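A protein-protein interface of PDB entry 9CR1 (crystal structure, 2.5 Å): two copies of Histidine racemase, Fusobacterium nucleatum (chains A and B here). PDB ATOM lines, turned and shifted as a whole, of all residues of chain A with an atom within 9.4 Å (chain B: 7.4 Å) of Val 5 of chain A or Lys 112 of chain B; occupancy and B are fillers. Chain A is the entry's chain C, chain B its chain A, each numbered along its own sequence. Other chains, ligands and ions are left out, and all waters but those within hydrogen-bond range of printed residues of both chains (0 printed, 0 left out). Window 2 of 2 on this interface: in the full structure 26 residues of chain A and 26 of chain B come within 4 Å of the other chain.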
ATOM      1  N   ASP A   2       2.875  22.314  31.607  1.00  0.00           N
ATOM      2  CA  ASP A   2       2.347  22.406  30.250  1.00  0.00           C
ATOM      3  C   ASP A   2       3.374  23.035  29.311  1.00  0.00           C
ATOM      4  O   ASP A   2       3.132  24.092  28.728  1.00  0.00           O
ATOM      5  CB  ASP A   2       1.050  23.217  30.236  1.00  0.00           C
ATOM      6  CG  ASP A   2       0.294  23.090  28.925  1.00  0.00           C
ATOM      7  OD1 ASP A   2       0.043  21.945  28.486  1.00  0.00           O
ATOM      8  OD2 ASP A   2      -0.050  24.135  28.333  1.00  0.00           O
ATOM      9  N   ARG A   3       4.526  22.380  29.172  1.00  0.00           N
ATOM     10  CA  ARG A   3       5.588  22.854  28.288  1.00  0.00           C
ATOM     11  C   ARG A   3       6.361  21.641  27.793  1.00  0.00           C
ATOM     12  O   ARG A   3       6.973  20.924  28.589  1.00  0.00           O
ATOM     13  CB  ARG A   3       6.503  23.857  29.006  1.00  0.00           C
ATOM     14  CG  ARG A   3       7.575  23.269  29.922  1.00  0.00           C
ATOM     15  CD  ARG A   3       6.981  22.497  31.089  1.00  0.00           C
ATOM     16  NE  ARG A   3       6.183  23.345  31.968  1.00  0.00           N
ATOM     17  CZ  ARG A   3       5.579  22.924  33.071  1.00  0.00           C
ATOM     18  NH1 ARG A   3       5.657  21.663  33.463  1.00  0.00           N
ATOM     19  NH2 ARG A   3       4.877  23.791  33.798  1.00  0.00           N
ATOM     20  N   LYS A   4       6.320  21.401  26.485  1.00  0.00           N
ATOM     21  CA  LYS A   4       6.881  20.188  25.910  1.00  0.00           C
ATOM     22  C   LYS A   4       7.296  20.462  24.474  1.00  0.00           C
ATOM     23  O   LYS A   4       6.481  20.926  23.672  1.00  0.00           O
ATOM     24  CB  LYS A   4       5.862  19.036  25.966  1.00  0.00           C
ATOM     25  CG  LYS A   4       4.459  19.409  25.482  1.00  0.00           C
ATOM     26  CD  LYS A   4       3.365  18.846  26.393  1.00  0.00           C
ATOM     27  CE  LYS A   4       1.988  19.380  26.004  1.00  0.00           C
ATOM     28  NZ  LYS A   4       1.068  19.526  27.170  1.00  0.00           N
ATOM     29  N   VAL A   5       8.558  20.177  24.155  1.00  0.00           N
ATOM     30  CA  VAL A   5       9.104  20.420  22.825  1.00  0.00           C
ATOM     31  C   VAL A   5       9.087  19.116  22.039  1.00  0.00           C
ATOM     32  O   VAL A   5       9.497  18.063  22.545  1.00  0.00           O
ATOM     33  CB  VAL A   5      10.527  21.004  22.897  1.00  0.00           C
ATOM     34  CG1 VAL A   5      10.549  22.262  23.768  1.00  0.00           C
ATOM     35  CG2 VAL A   5      11.511  19.966  23.419  1.00  0.00           C
ATOM     36  N   GLN A   6       8.609  19.185  20.803  1.00  0.00           N
ATOM     37  CA  GLN A   6       8.548  18.048  19.895  1.00  0.00           C
ATOM     38  C   GLN A   6       9.620  18.221  18.828  1.00  0.00           C
ATOM     39  O   GLN A   6       9.712  19.284  18.203  1.00  0.00           O
ATOM     40  CB  GLN A   6       7.160  17.949  19.262  1.00  0.00           C
ATOM     41  CG  GLN A   6       6.813  16.570  18.755  1.00  0.00           C
ATOM     42  CD  GLN A   6       5.328  16.401  18.500  1.00  0.00           C
ATOM     43  OE1 GLN A   6       4.548  17.343  18.648  1.00  0.00           O
ATOM     44  NE2 GLN A   6       4.930  15.194  18.119  1.00  0.00           N
ATOM     45  N   VAL A   7      10.433  17.186  18.630  1.00  0.00           N
ATOM     46  CA  VAL A   7      11.609  17.258  17.765  1.00  0.00           C
ATOM     47  C   VAL A   7      11.363  16.376  16.551  1.00  0.00           C
ATOM     48  O   VAL A   7      11.255  15.148  16.673  1.00  0.00           O
ATOM     49  CB  VAL A   7      12.888  16.838  18.502  1.00  0.00           C
ATOM     50  CG1 VAL A   7      14.122  17.130  17.652  1.00  0.00           C
ATOM     51  CG2 VAL A   7      12.981  17.551  19.846  1.00  0.00           C
ATOM     52  N   LEU A   8      11.287  16.999  15.379  1.00  0.00           N
ATOM     53  CA  LEU A   8      10.989  16.312  14.136  1.00  0.00           C
ATOM     54  C   LEU A   8      12.170  16.419  13.178  1.00  0.00           C
ATOM     55  O   LEU A   8      12.995  17.332  13.270  1.00  0.00           O
ATOM     56  CB  LEU A   8       9.732  16.901  13.479  1.00  0.00           C
ATOM     57  CG  LEU A   8       8.375  16.464  14.033  1.00  0.00           C
ATOM     58  CD1 LEU A   8       8.347  16.473  15.546  1.00  0.00           C
ATOM     59  CD2 LEU A   8       7.258  17.357  13.491  1.00  0.00           C
ATOM     60  N   LEU A  36       0.249  20.549  12.984  1.00  0.00           N
ATOM     61  CA  LEU A  36       1.700  20.609  12.862  1.00  0.00           C
ATOM     62  C   LEU A  36       2.108  21.232  11.533  1.00  0.00           C
ATOM     63  O   LEU A  36       3.056  22.021  11.472  1.00  0.00           O
ATOM     64  CB  LEU A  36       2.302  19.212  12.996  1.00  0.00           C
ATOM     65  CG  LEU A  36       2.231  18.528  14.361  1.00  0.00           C
ATOM     66  CD1 LEU A  36       3.086  17.259  14.344  1.00  0.00           C
ATOM     67  CD2 LEU A  36       2.665  19.453  15.482  1.00  0.00           C
ATOM     68  N   ILE A 261      13.633  20.206  13.696  1.00  0.00           N
ATOM     69  CA  ILE A 261      12.727  21.325  13.919  1.00  0.00           C
ATOM     70  C   ILE A 261      12.047  21.111  15.264  1.00  0.00           C
ATOM     71  O   ILE A 261      11.685  19.983  15.614  1.00  0.00           O
ATOM     72  CB  ILE A 261      11.694  21.457  12.780  1.00  0.00           C
ATOM     73  CG1 ILE A 261      10.580  22.423  13.170  1.00  0.00           C
ATOM     74  CG2 ILE A 261      11.123  20.101  12.425  1.00  0.00           C
ATOM     75  CD1 ILE A 261       9.725  22.867  12.010  1.00  0.00           C
ATOM     76  N   TYR A 262      11.885  22.190  16.024  1.00  0.00           N
ATOM     77  CA  TYR A 262      11.356  22.124  17.380  1.00  0.00           C
ATOM     78  C   TYR A 262       9.989  22.788  17.415  1.00  0.00           C
ATOM     79  O   TYR A 262       9.872  23.992  17.153  1.00  0.00           O
ATOM     80  CB  TYR A 262      12.302  22.798  18.374  1.00  0.00           C
ATOM     81  CG  TYR A 262      13.744  22.383  18.205  1.00  0.00           C
ATOM     82  CD1 TYR A 262      14.233  21.250  18.834  1.00  0.00           C
ATOM     83  CD2 TYR A 262      14.614  23.126  17.414  1.00  0.00           C
ATOM     84  CE1 TYR A 262      15.550  20.862  18.681  1.00  0.00           C
ATOM     85  CE2 TYR A 262      15.934  22.746  17.255  1.00  0.00           C
ATOM     86  CZ  TYR A 262      16.395  21.613  17.891  1.00  0.00           C
ATOM     87  OH  TYR A 262      17.707  21.219  17.744  1.00  0.00           O
ATOM     88  N   ILE A 263       8.965  22.006  17.745  1.00  0.00           N
ATOM     89  CA  ILE A 263       7.590  22.485  17.807  1.00  0.00           C
ATOM     90  C   ILE A 263       7.045  22.185  19.194  1.00  0.00           C
ATOM     91  O   ILE A 263       7.049  21.027  19.631  1.00  0.00           O
ATOM     92  CB  ILE A 263       6.706  21.838  16.732  1.00  0.00           C
ATOM     93  CG1 ILE A 263       7.380  21.920  15.366  1.00  0.00           C
ATOM     94  CG2 ILE A 263       5.340  22.508  16.694  1.00  0.00           C
ATOM     95  CD1 ILE A 263       7.779  20.571  14.817  1.00  0.00           C
ATOM     96  N   GLY A 264       6.579  23.222  19.883  1.00  0.00           N
ATOM     97  CA  GLY A 264       5.896  23.011  21.140  1.00  0.00           C
ATOM     98  C   GLY A 264       4.586  22.272  20.940  1.00  0.00           C
ATOM     99  O   GLY A 264       3.968  22.323  19.879  1.00  0.00           O
ATOM    100  N   LYS A 265       4.168  21.561  21.979  1.00  0.00           N
ATOM    101  CA  LYS A 265       2.922  20.794  21.936  1.00  0.00           C
ATOM    102  C   LYS A 265       2.079  21.195  23.146  1.00  0.00           C
ATOM    103  O   LYS A 265       2.554  21.903  24.038  1.00  0.00           O
ATOM    104  CB  LYS A 265       3.216  19.294  21.912  1.00  0.00           C
ATOM    105  CG  LYS A 265       2.023  18.393  22.201  1.00  0.00           C
ATOM    106  CD  LYS A 265       0.958  18.472  21.115  1.00  0.00           C
ATOM    107  CE  LYS A 265      -0.444  18.346  21.704  1.00  0.00           C
ATOM    108  NZ  LYS A 265      -0.818  19.529  22.533  1.00  0.00           N
ATOM    109  N   SER B  76      19.701  33.365  23.434  1.00  0.00           N
ATOM    110  CA  SER B  76      18.744  32.292  23.673  1.00  0.00           C
ATOM    111  C   SER B  76      19.268  30.962  23.153  1.00  0.00           C
ATOM    112  O   SER B  76      18.882  29.902  23.662  1.00  0.00           O
ATOM    113  CB  SER B  76      17.406  32.630  23.022  1.00  0.00           C
ATOM    114  OG  SER B  76      16.829  33.781  23.607  1.00  0.00           O
ATOM    115  N   ALA B  79      21.637  29.455  25.834  1.00  0.00           N
ATOM    116  CA  ALA B  79      20.864  28.833  26.899  1.00  0.00           C
ATOM    117  C   ALA B  79      20.304  27.498  26.442  1.00  0.00           C
ATOM    118  O   ALA B  79      20.335  26.513  27.190  1.00  0.00           O
ATOM    119  CB  ALA B  79      19.733  29.760  27.344  1.00  0.00           C
ATOM    120  N   PHE B  80      19.785  27.455  25.208  1.00  0.00           N
ATOM    121  CA  PHE B  80      19.263  26.221  24.632  1.00  0.00           C
ATOM    122  C   PHE B  80      20.299  25.108  24.661  1.00  0.00           C
ATOM    123  O   PHE B  80      19.941  23.933  24.814  1.00  0.00           O
ATOM    124  CB  PHE B  80      18.799  26.495  23.197  1.00  0.00           C
ATOM    125  CG  PHE B  80      17.885  25.445  22.628  1.00  0.00           C
ATOM    126  CD1 PHE B  80      16.657  25.182  23.218  1.00  0.00           C
ATOM    127  CD2 PHE B  80      18.245  24.733  21.491  1.00  0.00           C
ATOM    128  CE1 PHE B  80      15.811  24.217  22.692  1.00  0.00           C
ATOM    129  CE2 PHE B  80      17.401  23.769  20.964  1.00  0.00           C
ATOM    130  CZ  PHE B  80      16.184  23.513  21.565  1.00  0.00           C
ATOM    131  N   PHE B  85      21.552  25.574  32.219  1.00  0.00           N
ATOM    132  CA  PHE B  85      20.428  26.497  32.202  1.00  0.00           C
ATOM    133  C   PHE B  85      19.213  25.857  32.858  1.00  0.00           C
ATOM    134  O   PHE B  85      18.834  24.731  32.527  1.00  0.00           O
ATOM    135  CB  PHE B  85      20.082  26.908  30.775  1.00  0.00           C
ATOM    136  CG  PHE B  85      18.931  27.872  30.691  1.00  0.00           C
ATOM    137  CD1 PHE B  85      19.132  29.235  30.864  1.00  0.00           C
ATOM    138  CD2 PHE B  85      17.643  27.414  30.455  1.00  0.00           C
ATOM    139  CE1 PHE B  85      18.071  30.119  30.791  1.00  0.00           C
ATOM    140  CE2 PHE B  85      16.576  28.297  30.382  1.00  0.00           C
ATOM    141  CZ  PHE B  85      16.791  29.648  30.551  1.00  0.00           C
ATOM    142  N   SER B  86      18.605  26.584  33.797  1.00  0.00           N
ATOM    143  CA  SER B  86      17.381  26.138  34.439  1.00  0.00           C
ATOM    144  C   SER B  86      16.281  27.087  34.017  1.00  0.00           C
ATOM    145  O   SER B  86      15.665  26.890  32.949  1.00  0.00           O
ATOM    146  CB  SER B  86      17.574  26.054  35.960  1.00  0.00           C
ATOM    147  OG  SER B  86      18.171  27.238  36.450  1.00  0.00           O
ATOM    148  N   ASN B 108      13.418  31.436  30.718  1.00  0.00           N
ATOM    149  CA  ASN B 108      12.540  30.493  30.039  1.00  0.00           C
ATOM    150  C   ASN B 108      11.161  31.110  29.855  1.00  0.00           C
ATOM    151  O   ASN B 108      10.655  31.809  30.737  1.00  0.00           O
ATOM    152  CB  ASN B 108      12.424  29.193  30.831  1.00  0.00           C
ATOM    153  CG  ASN B 108      11.119  28.455  30.560  1.00  0.00           C
ATOM    154  OD1 ASN B 108      10.150  28.591  31.305  1.00  0.00           O
ATOM    155  ND2 ASN B 108      11.094  27.664  29.488  1.00  0.00           N
ATOM    156  N   ASP B 109      10.546  30.850  28.704  1.00  0.00           N
ATOM    157  CA  ASP B 109       9.237  31.402  28.364  1.00  0.00           C
ATOM    158  C   ASP B 109       8.285  30.261  27.981  1.00  0.00           C
ATOM    159  O   ASP B 109       7.690  30.246  26.911  1.00  0.00           O
ATOM    160  CB  ASP B 109       9.332  32.423  27.235  1.00  0.00           C
ATOM    161  CG  ASP B 109       8.104  33.319  27.151  1.00  0.00           C
ATOM    162  OD1 ASP B 109       7.455  33.544  28.188  1.00  0.00           O
ATOM    163  OD2 ASP B 109       7.796  33.807  26.033  1.00  0.00           O
ATOM    164  N   GLY B 110       8.142  29.293  28.884  1.00  0.00           N
ATOM    165  CA  GLY B 110       7.276  28.153  28.650  1.00  0.00           C
ATOM    166  C   GLY B 110       8.022  26.911  28.207  1.00  0.00           C
ATOM    167  O   GLY B 110       8.601  26.198  29.031  1.00  0.00           O
ATOM    168  N   ALA B 111       8.014  26.647  26.904  1.00  0.00           N
ATOM    169  CA  ALA B 111       8.680  25.476  26.357  1.00  0.00           C
ATOM    170  C   ALA B 111      10.199  25.628  26.414  1.00  0.00           C
ATOM    171  O   ALA B 111      10.739  26.728  26.565  1.00  0.00           O
ATOM    172  CB  ALA B 111       8.238  25.242  24.911  1.00  0.00           C
ATOM    173  N   LYS B 112      10.890  24.488  26.274  1.00  0.00           N
ATOM    174  CA  LYS B 112      12.347  24.483  26.339  1.00  0.00           C
ATOM    175  C   LYS B 112      12.983  25.223  25.169  1.00  0.00           C
ATOM    176  O   LYS B 112      14.132  25.665  25.273  1.00  0.00           O
ATOM    177  CB  LYS B 112      12.889  23.052  26.360  1.00  0.00           C
ATOM    178  CG  LYS B 112      12.238  22.122  27.352  1.00  0.00           C
ATOM    179  CD  LYS B 112      13.284  21.510  28.268  1.00  0.00           C
ATOM    180  CE  LYS B 112      12.662  21.046  29.576  1.00  0.00           C
ATOM    181  NZ  LYS B 112      13.703  20.743  30.601  1.00  0.00           N
ATOM    182  N   ASN B 113      12.284  25.312  24.040  1.00  0.00           N
ATOM    183  CA  ASN B 113      12.776  26.072  22.900  1.00  0.00           C
ATOM    184  C   ASN B 113      12.378  27.542  22.959  1.00  0.00           C
ATOM    185  O   ASN B 113      12.906  28.346  22.181  1.00  0.00           O
ATOM    186  CB  ASN B 113      12.272  25.449  21.591  1.00  0.00           C
ATOM    187  CG  ASN B 113      10.791  25.655  21.382  1.00  0.00           C
ATOM    188  OD1 ASN B 113       9.991  25.417  22.286  1.00  0.00           O
ATOM    189  ND2 ASN B 113      10.417  26.104  20.191  1.00  0.00           N
ATOM    190  N   LYS B 114      11.487  27.915  23.877  1.00  0.00           N
ATOM    191  CA  LYS B 114      11.017  29.286  24.022  1.00  0.00           C
ATOM    192  C   LYS B 114      11.735  29.971  25.175  1.00  0.00           C
ATOM    193  O   LYS B 114      12.001  29.361  26.215  1.00  0.00           O
ATOM    194  CB  LYS B 114       9.504  29.308  24.244  1.00  0.00           C
ATOM    195  CG  LYS B 114       8.710  29.439  22.946  1.00  0.00           C
ATOM    196  CD  LYS B 114       7.296  28.892  23.067  1.00  0.00           C
ATOM    197  CE  LYS B 114       6.309  29.978  23.479  1.00  0.00           C
ATOM    198  NZ  LYS B 114       5.322  29.463  24.474  1.00  0.00           N
ATOM    199  N   PHE B 115      12.059  31.246  24.980  1.00  0.00           N
ATOM    200  CA  PHE B 115      12.854  32.014  25.929  1.00  0.00           C
ATOM    201  C   PHE B 115      12.350  33.457  25.968  1.00  0.00           C
ATOM    202  O   PHE B 115      11.479  33.860  25.194  1.00  0.00           O
ATOM    203  CB  PHE B 115      14.347  32.016  25.557  1.00  0.00           C
ATOM    204  CG  PHE B 115      14.988  30.655  25.551  1.00  0.00           C
ATOM    205  CD1 PHE B 115      14.966  29.861  24.411  1.00  0.00           C
ATOM    206  CD2 PHE B 115      15.645  30.184  26.673  1.00  0.00           C
ATOM    207  CE1 PHE B 115      15.571  28.617  24.404  1.00  0.00           C
ATOM    208  CE2 PHE B 115      16.252  28.941  26.671  1.00  0.00           C
ATOM    209  CZ  PHE B 115      16.215  28.157  25.533  1.00  0.00           C
ATOM    210  N   ILE B 255      13.716  29.051  19.289  1.00  0.00           N
ATOM    211  CA  ILE B 255      14.593  28.295  18.401  1.00  0.00           C
ATOM    212  C   ILE B 255      13.719  27.441  17.494  1.00  0.00           C
ATOM    213  O   ILE B 255      12.996  26.555  17.964  1.00  0.00           O
ATOM    214  CB  ILE B 255      15.581  27.432  19.198  1.00  0.00           C
ATOM    215  CG1 ILE B 255      16.232  28.250  20.315  1.00  0.00           C
ATOM    216  CG2 ILE B 255      16.648  26.860  18.269  1.00  0.00           C
ATOM    217  CD1 ILE B 255      17.342  29.187  19.843  1.00  0.00           C
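Printed residues of chain B within 4 Å of Arg 3 of chain A: Gly 110 and Ala 111.
Of chain B, only Ala 111, Lys 112 and Asn 113 come within 4 Å of Val 5 of chain A.
Leu 36 of chain A touches none of the printed residues of chain B.
Printed residues of chain B within 4 Å of Tyr 262 of chain A: Phe 80 (3.9 Å), Asn 113 (3.7 Å) and Ile 255 (3.8 Å).
Ile 263 of chain A touches none of the printed residues of chain B.
Of the printed residues of chain A, Phe 80 of chain B touches Tyr 262 (3.9 Å).
Of chain A, only Arg 3 and Val 5 come within 4 Å of Ala 111 of chain B.
Lys 112 of chain B touches just one residue of chain A: Val 5.
Asn 113 of chain B touches just these residues of chain A: Val 5 and Tyr 262.
Of the printed residues of chain A, Ile 255 of chain B touches Tyr 262.
The nearest printed residue of chain B that does not touch Val 5 of chain A is Phe 80 of chain B (5.7 Å).
Of the 14 printed residues of chain B, 6 touch a printed residue of chain A.
Printed residues of chain B that touch a printed residue of chain A: Phe 80, Gly 110, Ala 111, Lys 112, Asn 113 and Ile 255.
Hydrophobic or aromatic side chains of chain B that line the printed part of chain A: Phe 80 and Ala 111.
Hydrophobic or aromatic side chains of chain A within 4 Å of the printed part of chain B: Val 5 and Tyr 262.
Along chain A the printed residues that touch a printed residue of chain B span positions 3 to 262.
Among the printed residues, 8 pairs touch across the chains.
Among the printed residues, no Asp or Glu carboxylate lies within 4 Å of a Lys or Arg side-chain nitrogen of the other chain.
Among the printed residues, pairs that only touch across the chains: Arg 3 of chain A with Gly 110 of chain B (3.1 Å), Val 5 of chain A with Lys 112 of chain B (3.4 Å), Val 5 of chain A with Asn 113 of chain B (3.5 Å), Tyr 262 of chain A with Asn 113 of chain B (3.7 Å), Arg 3 of chain A with Ala 111 of chain B (3.8 Å), Tyr 262 of chain A with Ile 255 of chain B (3.8 Å), Tyr 262 of chain A with Phe 80 of chain B (3.9 Å) and Val 5 of chain A with Ala 111 of chain B (3.9 Å).
The backbone carbonyl oxygen (O) of Gly 110 of chain B lies within hydrogen-bond range of the side-chain amide nitrogen (ND2) of Asn 108 of chain B (2.9 Å).
O of Ala 111 of chain B is in hydrogen-bond range of ND2 of Asn 108 of chain B (3.1 Å).
O of Asn 113 of chain B lies within hydrogen-bond range of N of Ile 255 of chain B, 3.1 Å away.
No position is printed for both chains.
Of the 8 pairs that touch across the chains among the printed residues, none has its exchanged pair printed and touching as well.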
